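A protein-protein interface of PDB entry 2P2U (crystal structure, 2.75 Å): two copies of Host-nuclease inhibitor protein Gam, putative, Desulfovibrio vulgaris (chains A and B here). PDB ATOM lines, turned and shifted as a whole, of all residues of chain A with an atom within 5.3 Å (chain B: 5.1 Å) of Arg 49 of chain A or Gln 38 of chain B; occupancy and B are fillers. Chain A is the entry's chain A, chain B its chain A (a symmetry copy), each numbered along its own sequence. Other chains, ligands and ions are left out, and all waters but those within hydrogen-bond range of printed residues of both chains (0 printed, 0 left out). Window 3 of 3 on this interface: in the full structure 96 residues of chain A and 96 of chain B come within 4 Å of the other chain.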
ATOM      1  N   ALA A  45     -30.233  11.910 -11.396  1.00  0.00           N
ATOM      2  CA  ALA A  45     -28.939  11.666 -12.005  1.00  0.00           C
ATOM      3  C   ALA A  45     -29.044  11.605 -13.547  1.00  0.00           C
ATOM      4  O   ALA A  45     -28.162  12.092 -14.275  1.00  0.00           O
ATOM      5  CB  ALA A  45     -28.341  10.388 -11.465  1.00  0.00           C
ATOM      6  N   ALA A  46     -30.121  11.012 -14.046  1.00  0.00           N
ATOM      7  CA  ALA A  46     -30.256  10.881 -15.461  1.00  0.00           C
ATOM      8  C   ALA A  46     -30.427  12.284 -16.036  1.00  0.00           C
ATOM      9  O   ALA A  46     -29.703  12.645 -16.949  1.00  0.00           O
ATOM     10  CB  ALA A  46     -31.405   9.947 -15.823  1.00  0.00           C
ATOM     11  N   LYS A  47     -31.321  13.094 -15.475  1.00  0.00           N
ATOM     12  CA  LYS A  47     -31.556  14.429 -16.015  1.00  0.00           C
ATOM     13  C   LYS A  47     -30.270  15.235 -16.020  1.00  0.00           C
ATOM     14  O   LYS A  47     -30.137  16.198 -16.765  1.00  0.00           O
ATOM     15  CB  LYS A  47     -32.628  15.183 -15.226  1.00  0.00           C
ATOM     16  CG  LYS A  47     -34.046  14.785 -15.563  1.00  0.00           C
ATOM     17  CD  LYS A  47     -35.092  15.761 -14.963  1.00  0.00           C
ATOM     18  CE  LYS A  47     -36.491  15.091 -14.965  1.00  0.00           C
ATOM     19  NZ  LYS A  47     -37.658  15.909 -14.550  1.00  0.00           N
ATOM     20  N   ALA A  48     -29.317  14.836 -15.192  1.00  0.00           N
ATOM     21  CA  ALA A  48     -28.110  15.617 -14.989  1.00  0.00           C
ATOM     22  C   ALA A  48     -27.022  15.181 -15.968  1.00  0.00           C
ATOM     23  O   ALA A  48     -26.249  16.018 -16.436  1.00  0.00           O
ATOM     24  CB  ALA A  48     -27.629  15.489 -13.542  1.00  0.00           C
ATOM     25  N   ARG A  49     -26.945  13.875 -16.253  1.00  0.00           N
ATOM     26  CA  ARG A  49     -26.080  13.348 -17.317  1.00  0.00           C
ATOM     27  C   ARG A  49     -26.539  13.900 -18.687  1.00  0.00           C
ATOM     28  O   ARG A  49     -25.715  14.431 -19.458  1.00  0.00           O
ATOM     29  CB  ARG A  49     -26.139  11.814 -17.383  1.00  0.00           C
ATOM     30  CG  ARG A  49     -25.043  10.955 -16.713  1.00  0.00           C
ATOM     31  CD  ARG A  49     -25.273   9.440 -17.099  1.00  0.00           C
ATOM     32  NE  ARG A  49     -26.651   9.163 -17.611  1.00  0.00           N
ATOM     33  CZ  ARG A  49     -27.115   7.996 -18.105  1.00  0.00           C
ATOM     34  NH1 ARG A  49     -26.322   6.922 -18.171  1.00  0.00           N
ATOM     35  NH2 ARG A  49     -28.386   7.905 -18.544  1.00  0.00           N
ATOM     36  N   ALA A  50     -27.843  13.765 -18.976  1.00  0.00           N
ATOM     37  CA  ALA A  50     -28.413  14.175 -20.254  1.00  0.00           C
ATOM     38  C   ALA A  50     -27.954  15.588 -20.533  1.00  0.00           C
ATOM     39  O   ALA A  50     -27.134  15.818 -21.444  1.00  0.00           O
ATOM     40  CB  ALA A  50     -29.921  14.100 -20.235  1.00  0.00           C
ATOM     41  N   SER A  51     -28.454  16.506 -19.706  1.00  0.00           N
ATOM     42  CA  SER A  51     -28.100  17.918 -19.742  1.00  0.00           C
ATOM     43  C   SER A  51     -26.584  18.255 -19.573  1.00  0.00           C
ATOM     44  O   SER A  51     -26.141  19.325 -20.011  1.00  0.00           O
ATOM     45  CB  SER A  51     -28.955  18.675 -18.730  1.00  0.00           C
ATOM     46  OG  SER A  51     -28.353  19.956 -18.470  1.00  0.00           O
ATOM     47  N   GLN A  52     -25.788  17.357 -18.986  1.00  0.00           N
ATOM     48  CA  GLN A  52     -24.306  17.540 -18.986  1.00  0.00           C
ATOM     49  C   GLN A  52     -23.715  17.349 -20.386  1.00  0.00           C
ATOM     50  O   GLN A  52     -22.999  18.215 -20.871  1.00  0.00           O
ATOM     51  CB  GLN A  52     -23.585  16.586 -18.008  1.00  0.00           C
ATOM     52  CG  GLN A  52     -22.027  16.681 -18.005  1.00  0.00           C
ATOM     53  CD  GLN A  52     -21.277  15.294 -17.889  1.00  0.00           C
ATOM     54  OE1 GLN A  52     -21.532  14.355 -18.666  1.00  0.00           O
ATOM     55  NE2 GLN A  52     -20.331  15.198 -16.937  1.00  0.00           N
ATOM     56  N   LYS A  53     -24.005  16.216 -21.024  1.00  0.00           N
ATOM     57  CA  LYS A  53     -23.478  15.939 -22.353  1.00  0.00           C
ATOM     58  C   LYS A  53     -24.053  16.848 -23.455  1.00  0.00           C
ATOM     59  O   LYS A  53     -23.367  17.101 -24.438  1.00  0.00           O
ATOM     60  CB  LYS A  53     -23.677  14.464 -22.749  1.00  0.00           C
ATOM     61  CG  LYS A  53     -23.013  13.414 -21.842  1.00  0.00           C
ATOM     62  CD  LYS A  53     -21.614  13.019 -22.308  1.00  0.00           C
ATOM     63  CE  LYS A  53     -20.839  12.311 -21.188  1.00  0.00           C
ATOM     64  NZ  LYS A  53     -19.373  12.276 -21.445  1.00  0.00           N
ATOM     65  N   SER A  54     -25.283  17.341 -23.325  1.00  0.00           N
ATOM     66  CA  SER A  54     -25.886  18.058 -24.458  1.00  0.00           C
ATOM     67  C   SER A  54     -25.839  19.582 -24.372  1.00  0.00           C
ATOM     68  O   SER A  54     -26.294  20.294 -25.276  1.00  0.00           O
ATOM     69  CB  SER A  54     -27.303  17.573 -24.743  1.00  0.00           C
ATOM     70  OG  SER A  54     -28.239  18.201 -23.899  1.00  0.00           O
ATOM     71  N   GLU B  34     -30.633  11.474 -29.058  1.00  0.00           N
ATOM     72  CA  GLU B  34     -30.310  10.118 -28.654  1.00  0.00           C
ATOM     73  C   GLU B  34     -29.696  10.066 -27.253  1.00  0.00           C
ATOM     74  O   GLU B  34     -29.766   9.032 -26.565  1.00  0.00           O
ATOM     75  CB  GLU B  34     -29.381   9.489 -29.679  1.00  0.00           C
ATOM     76  CG  GLU B  34     -28.153   8.775 -29.124  1.00  0.00           C
ATOM     77  CD  GLU B  34     -27.091   8.506 -30.199  1.00  0.00           C
ATOM     78  OE1 GLU B  34     -25.871   8.701 -29.866  1.00  0.00           O
ATOM     79  OE2 GLU B  34     -27.476   8.116 -31.364  1.00  0.00           O
ATOM     80  N   ILE B  35     -29.062  11.165 -26.847  1.00  0.00           N
ATOM     81  CA  ILE B  35     -28.820  11.457 -25.424  1.00  0.00           C
ATOM     82  C   ILE B  35     -30.172  11.349 -24.687  1.00  0.00           C
ATOM     83  O   ILE B  35     -30.294  10.630 -23.700  1.00  0.00           O
ATOM     84  CB  ILE B  35     -28.205  12.878 -25.266  1.00  0.00           C
ATOM     85  CG1 ILE B  35     -26.677  12.834 -25.256  1.00  0.00           C
ATOM     86  CG2 ILE B  35     -28.747  13.611 -24.031  1.00  0.00           C
ATOM     87  CD1 ILE B  35     -26.059  14.226 -25.245  1.00  0.00           C
ATOM     88  N   GLU B  36     -31.177  12.031 -25.239  1.00  0.00           N
ATOM     89  CA  GLU B  36     -32.551  12.055 -24.756  1.00  0.00           C
ATOM     90  C   GLU B  36     -33.331  10.758 -24.980  1.00  0.00           C
ATOM     91  O   GLU B  36     -34.535  10.711 -24.786  1.00  0.00           O
ATOM     92  CB  GLU B  36     -33.311  13.241 -25.394  1.00  0.00           C
ATOM     93  CG  GLU B  36     -33.156  14.573 -24.621  1.00  0.00           C
ATOM     94  CD  GLU B  36     -33.312  15.821 -25.486  1.00  0.00           C
ATOM     95  OE1 GLU B  36     -33.903  15.709 -26.580  1.00  0.00           O
ATOM     96  OE2 GLU B  36     -32.849  16.920 -25.076  1.00  0.00           O
ATOM     97  N   ALA B  37     -32.678   9.704 -25.412  1.00  0.00           N
ATOM     98  CA  ALA B  37     -33.377   8.437 -25.523  1.00  0.00           C
ATOM     99  C   ALA B  37     -32.873   7.659 -24.339  1.00  0.00           C
ATOM    100  O   ALA B  37     -33.623   6.946 -23.688  1.00  0.00           O
ATOM    101  CB  ALA B  37     -33.028   7.721 -26.844  1.00  0.00           C
ATOM    102  N   GLN B  38     -31.585   7.833 -24.064  1.00  0.00           N
ATOM    103  CA  GLN B  38     -30.922   7.184 -22.950  1.00  0.00           C
ATOM    104  C   GLN B  38     -31.414   7.635 -21.568  1.00  0.00           C
ATOM    105  O   GLN B  38     -31.381   6.877 -20.599  1.00  0.00           O
ATOM    106  CB  GLN B  38     -29.437   7.459 -23.043  1.00  0.00           C
ATOM    107  CG  GLN B  38     -28.803   6.657 -24.109  1.00  0.00           C
ATOM    108  CD  GLN B  38     -27.330   6.591 -23.908  1.00  0.00           C
ATOM    109  OE1 GLN B  38     -26.849   6.710 -22.773  1.00  0.00           O
ATOM    110  NE2 GLN B  38     -26.586   6.412 -25.000  1.00  0.00           N
ATOM    111  N   MET B  39     -31.815   8.893 -21.487  1.00  0.00           N
ATOM    112  CA  MET B  39     -32.304   9.460 -20.259  1.00  0.00           C
ATOM    113  C   MET B  39     -33.674   8.835 -19.984  1.00  0.00           C
ATOM    114  O   MET B  39     -33.922   8.367 -18.865  1.00  0.00           O
ATOM    115  CB  MET B  39     -32.368  10.979 -20.395  1.00  0.00           C
ATOM    116  CG  MET B  39     -32.964  11.708 -19.245  1.00  0.00           C
ATOM    117  SD  MET B  39     -33.407  13.553 -19.748  1.00  0.00           S
ATOM    118  CE  MET B  39     -35.224  13.492 -20.535  1.00  0.00           C
ATOM    119  N   ASN B  40     -34.525   8.794 -21.012  1.00  0.00           N
ATOM    120  CA  ASN B  40     -35.853   8.202 -20.934  1.00  0.00           C
ATOM    121  C   ASN B  40     -35.847   6.670 -20.842  1.00  0.00           C
ATOM    122  O   ASN B  40     -36.902   6.030 -20.750  1.00  0.00           O
ATOM    123  CB  ASN B  40     -36.679   8.651 -22.128  1.00  0.00           C
ATOM    124  CG  ASN B  40     -37.079  10.103 -22.052  1.00  0.00           C
ATOM    125  OD1 ASN B  40     -36.526  10.882 -21.279  1.00  0.00           O
ATOM    126  ND2 ASN B  40     -38.053  10.477 -22.851  1.00  0.00           N
ATOM    127  N   GLU B  41     -34.661   6.077 -20.899  1.00  0.00           N
ATOM    128  CA  GLU B  41     -34.502   4.671 -20.592  1.00  0.00           C
ATOM    129  C   GLU B  41     -34.040   4.508 -19.131  1.00  0.00           C
ATOM    130  O   GLU B  41     -34.324   3.497 -18.486  1.00  0.00           O
ATOM    131  CB  GLU B  41     -33.498   4.046 -21.563  1.00  0.00           C
ATOM    132  CG  GLU B  41     -32.885   2.677 -21.158  1.00  0.00           C
ATOM    133  CD  GLU B  41     -32.135   2.005 -22.313  1.00  0.00           C
ATOM    134  OE1 GLU B  41     -32.598   0.944 -22.787  1.00  0.00           O
ATOM    135  OE2 GLU B  41     -31.097   2.552 -22.771  1.00  0.00           O
ATOM    136  N   ALA B  42     -33.320   5.509 -18.623  1.00  0.00           N
ATOM    137  CA  ALA B  42     -32.823   5.500 -17.256  1.00  0.00           C
ATOM    138  C   ALA B  42     -33.981   5.809 -16.293  1.00  0.00           C
ATOM    139  O   ALA B  42     -34.128   5.147 -15.245  1.00  0.00           O
ATOM    140  CB  ALA B  42     -31.681   6.490 -17.094  1.00  0.00           C
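Among the printed residues, merely in contact across the chains: Ala 46 of chain A with Ala 42 of chain B, Arg 49 of chain A with Gln 38 of chain B, Arg 49 of chain A with Ala 42 of chain B, Ala 50 of chain A with Ile 35 of chain B, Ala 50 of chain A with Met 39 of chain B, Lys 53 of chain A with Ile 35 of chain B and Ser 54 of chain A with Ile 35 of chain B.
Arg 49 of chain A touches just these residues of chain B: Gln 38 and Ala 42.
Printed residues of chain B within 4 Å of Ser 54 of chain A: Ile 35 (3.6 Å).
Of the printed residues of chain A, Ile 35 of chain B touches Ala 50 (3.8 Å), Lys 53 (3.5 Å) and Ser 54 (3.6 Å).
Glu 36 of chain B touches none of the printed residues of chain A.
Ala 37 of chain B touches none of the printed residues of chain A.
Of chain A, only Arg 49 (3.8 Å) comes within 4 Å of Gln 38 of chain B.
Printed residues of chain A within 4 Å of Met 39 of chain B: Ala 50 (3.6 Å).
The nearest residue of chain B that does not touch Arg 49 of chain A is Met 39 of chain B (4.6 Å).
The nearest printed residue of chain B that does not touch Ser 54 of chain A is Glu 36 of chain B (4.9 Å).
Hydrophobic or aromatic side chains of chain A that line the printed part of chain B: Ala 46 and Ala 50.
Printed residues of chain B that touch a printed residue of chain A: Ile 35, Gln 38, Met 39 and Ala 42.
Hydrophobic or aromatic side chains of chain B that line the printed part of chain A: Ile 35, Met 39 and Ala 42.
Among the printed residues, 7 pairs touch across the chains.
No position is printed for both chains.
Of the 7 pairs that touch across the chains among the printed residues, none has its exchanged pair printed and touching as well.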
